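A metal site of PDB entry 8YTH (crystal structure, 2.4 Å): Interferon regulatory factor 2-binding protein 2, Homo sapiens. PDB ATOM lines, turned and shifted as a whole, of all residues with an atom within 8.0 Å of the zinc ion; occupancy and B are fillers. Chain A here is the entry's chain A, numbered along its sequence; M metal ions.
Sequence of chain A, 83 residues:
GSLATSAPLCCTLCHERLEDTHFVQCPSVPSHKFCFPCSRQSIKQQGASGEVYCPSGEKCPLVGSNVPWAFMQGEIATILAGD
Four residues have an atom within 4 Å of the zinc ion: Cys 11, Cys 14, Cys 35 and Cys 38. The nearest printed residue that does not touch the zinc ion is Leu 13 (4.6 Å).
The zinc ion is bound by the side-chain sulfur of Cys 38 (2.3 Å), the side-chain sulfur of Cys 35 (2.3 Å), the side-chain sulfur of Cys 14 (2.3 Å) and the side-chain sulfur of Cys 11 (2.4 Å). The zinc ion has four donor atoms within binding distance.
SG of Cys 14 lies close to N of Glu 16, at 3.4 Å. A ring nitrogen (ND1) of His 15 sits close to the backbone carbonyl oxygen (O) of Cys 11 (3.5 Å). SG of Cys 11 lies close to N of Leu 13, 3.4 Å away. O of Glu 16 is in hydrogen-bond range of N of Cys 11. The backbone carbonyl oxygen (O) of Cys 35 sits at hydrogen-bond distance from the side-chain hydroxyl (OG) of Ser 39.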
ATOM      1  N   CYS A  10     -12.517  26.611 -14.790  1.00  0.00           N
ATOM      2  CA  CYS A  10     -13.523  25.658 -15.232  1.00  0.00           C
ATOM      3  C   CYS A  10     -13.334  24.375 -14.447  1.00  0.00           C
ATOM      4  O   CYS A  10     -12.301  24.146 -13.820  1.00  0.00           O
ATOM      5  CB  CYS A  10     -13.464  25.441 -16.757  1.00  0.00           C
ATOM      6  SG  CYS A  10     -12.645  24.001 -17.399  1.00  0.00           S
ATOM      7  N   CYS A  11     -14.386  23.561 -14.450  1.00  0.00           N
ATOM      8  CA  CYS A  11     -14.492  22.417 -13.561  1.00  0.00           C
ATOM      9  C   CYS A  11     -13.456  21.367 -13.940  1.00  0.00           C
ATOM     10  O   CYS A  11     -13.289  21.037 -15.108  1.00  0.00           O
ATOM     11  CB  CYS A  11     -15.900  21.841 -13.633  1.00  0.00           C
ATOM     12  SG  CYS A  11     -16.178  20.375 -12.635  1.00  0.00           S
ATOM     13  N   THR A  12     -12.729  20.849 -12.941  1.00  0.00           N
ATOM     14  CA  THR A  12     -11.685  19.900 -13.301  1.00  0.00           C
ATOM     15  C   THR A  12     -12.232  18.497 -13.534  1.00  0.00           C
ATOM     16  O   THR A  12     -11.455  17.557 -13.732  1.00  0.00           O
ATOM     17  CB  THR A  12     -10.589  19.890 -12.240  1.00  0.00           C
ATOM     18  OG1 THR A  12      -9.516  19.041 -12.662  1.00  0.00           O
ATOM     19  CG2 THR A  12     -11.123  19.384 -10.913  1.00  0.00           C
ATOM     20  N   LEU A  13     -13.556  18.346 -13.498  1.00  0.00           N
ATOM     21  CA  LEU A  13     -14.225  17.079 -13.790  1.00  0.00           C
ATOM     22  C   LEU A  13     -15.003  17.150 -15.102  1.00  0.00           C
ATOM     23  O   LEU A  13     -14.753  16.358 -16.026  1.00  0.00           O
ATOM     24  CB  LEU A  13     -15.157  16.689 -12.647  1.00  0.00           C
ATOM     25  CG  LEU A  13     -14.523  16.547 -11.264  1.00  0.00           C
ATOM     26  CD1 LEU A  13     -15.549  16.055 -10.240  1.00  0.00           C
ATOM     27  CD2 LEU A  13     -13.322  15.629 -11.308  1.00  0.00           C
ATOM     28  N   CYS A  14     -15.954  18.067 -15.212  1.00  0.00           N
ATOM     29  CA  CYS A  14     -16.769  18.180 -16.419  1.00  0.00           C
ATOM     30  C   CYS A  14     -16.256  19.257 -17.374  1.00  0.00           C
ATOM     31  O   CYS A  14     -16.674  19.272 -18.540  1.00  0.00           O
ATOM     32  CB  CYS A  14     -18.220  18.488 -16.047  1.00  0.00           C
ATOM     33  SG  CYS A  14     -18.552  20.229 -15.715  1.00  0.00           S
ATOM     34  N   HIS A  15     -15.368  20.137 -16.906  1.00  0.00           N
ATOM     35  CA  HIS A  15     -14.721  21.146 -17.745  1.00  0.00           C
ATOM     36  C   HIS A  15     -15.716  22.166 -18.292  1.00  0.00           C
ATOM     37  O   HIS A  15     -15.598  22.655 -19.413  1.00  0.00           O
ATOM     38  CB  HIS A  15     -13.906  20.501 -18.868  1.00  0.00           C
ATOM     39  CG  HIS A  15     -12.817  19.610 -18.376  1.00  0.00           C
ATOM     40  ND1 HIS A  15     -11.587  20.079 -17.972  1.00  0.00           N
ATOM     41  CD2 HIS A  15     -12.796  18.266 -18.171  1.00  0.00           C
ATOM     42  CE1 HIS A  15     -10.835  19.067 -17.583  1.00  0.00           C
ATOM     43  NE2 HIS A  15     -11.555  17.955 -17.684  1.00  0.00           N
ATOM     44  N   GLU A  16     -16.702  22.504 -17.470  1.00  0.00           N
ATOM     45  CA  GLU A  16     -17.602  23.607 -17.756  1.00  0.00           C
ATOM     46  C   GLU A  16     -17.015  24.885 -17.172  1.00  0.00           C
ATOM     47  O   GLU A  16     -16.448  24.869 -16.072  1.00  0.00           O
ATOM     48  CB  GLU A  16     -18.989  23.333 -17.161  1.00  0.00           C
ATOM     49  CG  GLU A  16     -19.605  24.497 -16.429  1.00  0.00           C
ATOM     50  CD  GLU A  16     -20.773  25.107 -17.181  1.00  0.00           C
ATOM     51  OE1 GLU A  16     -21.227  24.479 -18.169  1.00  0.00           O
ATOM     52  OE2 GLU A  16     -21.225  26.198 -16.788  1.00  0.00           O
ATOM     53  N   ARG A  17     -17.114  25.981 -17.914  1.00  0.00           N
ATOM     54  CA  ARG A  17     -16.551  27.246 -17.444  1.00  0.00           C
ATOM     55  C   ARG A  17     -17.292  27.717 -16.200  1.00  0.00           C
ATOM     56  O   ARG A  17     -18.465  27.413 -15.979  1.00  0.00           O
ATOM     57  CB  ARG A  17     -16.609  28.313 -18.544  1.00  0.00           C
ATOM     58  CG  ARG A  17     -15.869  27.941 -19.836  1.00  0.00           C
ATOM     59  CD  ARG A  17     -14.410  27.524 -19.590  1.00  0.00           C
ATOM     60  NE  ARG A  17     -13.645  28.519 -18.841  1.00  0.00           N
ATOM     61  CZ  ARG A  17     -12.326  28.511 -18.708  1.00  0.00           C
ATOM     62  NH1 ARG A  17     -11.586  27.582 -19.289  1.00  0.00           N
ATOM     63  NH2 ARG A  17     -11.738  29.449 -17.967  1.00  0.00           N
ATOM     64  N   LEU A  18     -16.565  28.447 -15.345  1.00  0.00           N
ATOM     65  CA  LEU A  18     -17.057  28.915 -14.058  1.00  0.00           C
ATOM     66  C   LEU A  18     -16.851  30.414 -13.925  1.00  0.00           C
ATOM     67  O   LEU A  18     -16.603  30.946 -12.844  1.00  0.00           O
ATOM     68  CB  LEU A  18     -16.336  28.181 -12.913  1.00  0.00           C
ATOM     69  CG  LEU A  18     -16.195  26.665 -13.089  1.00  0.00           C
ATOM     70  CD1 LEU A  18     -15.321  26.061 -12.004  1.00  0.00           C
ATOM     71  CD2 LEU A  18     -17.575  25.995 -13.112  1.00  0.00           C
ATOM     72  N   LYS A  33     -11.136  22.947  -8.994  1.00  0.00           N
ATOM     73  CA  LYS A  33     -12.408  23.645  -9.080  1.00  0.00           C
ATOM     74  C   LYS A  33     -13.490  22.701  -9.587  1.00  0.00           C
ATOM     75  O   LYS A  33     -13.235  21.857 -10.451  1.00  0.00           O
ATOM     76  CB  LYS A  33     -12.315  24.873 -10.003  1.00  0.00           C
ATOM     77  CG  LYS A  33     -11.499  25.998  -9.397  1.00  0.00           C
ATOM     78  CD  LYS A  33     -11.345  27.147 -10.365  1.00  0.00           C
ATOM     79  CE  LYS A  33      -9.906  27.602 -10.387  1.00  0.00           C
ATOM     80  NZ  LYS A  33      -9.407  27.872  -9.009  1.00  0.00           N
ATOM     81  N   PHE A  34     -14.699  22.837  -9.026  1.00  0.00           N
ATOM     82  CA  PHE A  34     -15.800  21.947  -9.327  1.00  0.00           C
ATOM     83  C   PHE A  34     -17.088  22.745  -9.445  1.00  0.00           C
ATOM     84  O   PHE A  34     -17.389  23.562  -8.575  1.00  0.00           O
ATOM     85  CB  PHE A  34     -15.970  20.872  -8.241  1.00  0.00           C
ATOM     86  CG  PHE A  34     -14.683  20.248  -7.776  1.00  0.00           C
ATOM     87  CD1 PHE A  34     -14.094  19.213  -8.488  1.00  0.00           C
ATOM     88  CD2 PHE A  34     -14.071  20.695  -6.612  1.00  0.00           C
ATOM     89  CE1 PHE A  34     -12.907  18.636  -8.052  1.00  0.00           C
ATOM     90  CE2 PHE A  34     -12.879  20.125  -6.171  1.00  0.00           C
ATOM     91  CZ  PHE A  34     -12.305  19.101  -6.900  1.00  0.00           C
ATOM     92  N   CYS A  35     -17.855  22.500 -10.502  1.00  0.00           N
ATOM     93  CA  CYS A  35     -19.162  23.122 -10.611  1.00  0.00           C
ATOM     94  C   CYS A  35     -20.100  22.539  -9.567  1.00  0.00           C
ATOM     95  O   CYS A  35     -19.843  21.498  -8.950  1.00  0.00           O
ATOM     96  CB  CYS A  35     -19.742  22.910 -12.011  1.00  0.00           C
ATOM     97  SG  CYS A  35     -19.996  21.181 -12.442  1.00  0.00           S
ATOM     98  N   PHE A  36     -21.220  23.221  -9.350  1.00  0.00           N
ATOM     99  CA  PHE A  36     -22.175  22.718  -8.368  1.00  0.00           C
ATOM    100  C   PHE A  36     -22.730  21.338  -8.739  1.00  0.00           C
ATOM    101  O   PHE A  36     -22.764  20.464  -7.862  1.00  0.00           O
ATOM    102  CB  PHE A  36     -23.281  23.744  -8.135  1.00  0.00           C
ATOM    103  CG  PHE A  36     -23.009  24.651  -6.972  1.00  0.00           C
ATOM    104  CD1 PHE A  36     -21.776  25.258  -6.845  1.00  0.00           C
ATOM    105  CD2 PHE A  36     -23.972  24.879  -5.996  1.00  0.00           C
ATOM    106  CE1 PHE A  36     -21.503  26.086  -5.776  1.00  0.00           C
ATOM    107  CE2 PHE A  36     -23.706  25.711  -4.923  1.00  0.00           C
ATOM    108  CZ  PHE A  36     -22.464  26.310  -4.817  1.00  0.00           C
ATOM    109  N   PRO A  37     -23.131  21.070  -9.991  1.00  0.00           N
ATOM    110  CA  PRO A  37     -23.546  19.690 -10.320  1.00  0.00           C
ATOM    111  C   PRO A  37     -22.514  18.638  -9.989  1.00  0.00           C
ATOM    112  O   PRO A  37     -22.859  17.616  -9.384  1.00  0.00           O
ATOM    113  CB  PRO A  37     -23.828  19.782 -11.827  1.00  0.00           C
ATOM    114  CG  PRO A  37     -24.297  21.162 -12.018  1.00  0.00           C
ATOM    115  CD  PRO A  37     -23.429  21.996 -11.099  1.00  0.00           C
ATOM    116  N   CYS A  38     -21.237  18.862 -10.340  1.00  0.00           N
ATOM    117  CA  CYS A  38     -20.212  17.880 -10.013  1.00  0.00           C
ATOM    118  C   CYS A  38     -20.022  17.747  -8.507  1.00  0.00           C
ATOM    119  O   CYS A  38     -19.788  16.640  -7.998  1.00  0.00           O
ATOM    120  CB  CYS A  38     -18.885  18.245 -10.696  1.00  0.00           C
ATOM    121  SG  CYS A  38     -18.737  17.802 -12.461  1.00  0.00           S
ATOM    122  N   SER A  39     -20.115  18.859  -7.771  1.00  0.00           N
ATOM    123  CA  SER A  39     -20.052  18.764  -6.314  1.00  0.00           C
ATOM    124  C   SER A  39     -21.236  18.000  -5.747  1.00  0.00           C
ATOM    125  O   SER A  39     -21.078  17.228  -4.799  1.00  0.00           O
ATOM    126  CB  SER A  39     -19.982  20.167  -5.697  1.00  0.00           C
ATOM    127  OG  SER A  39     -18.882  20.897  -6.207  1.00  0.00           O
HETATM  128 ZN    ZN M   1     -18.346  19.870 -13.413  1.00  0.00          ZN
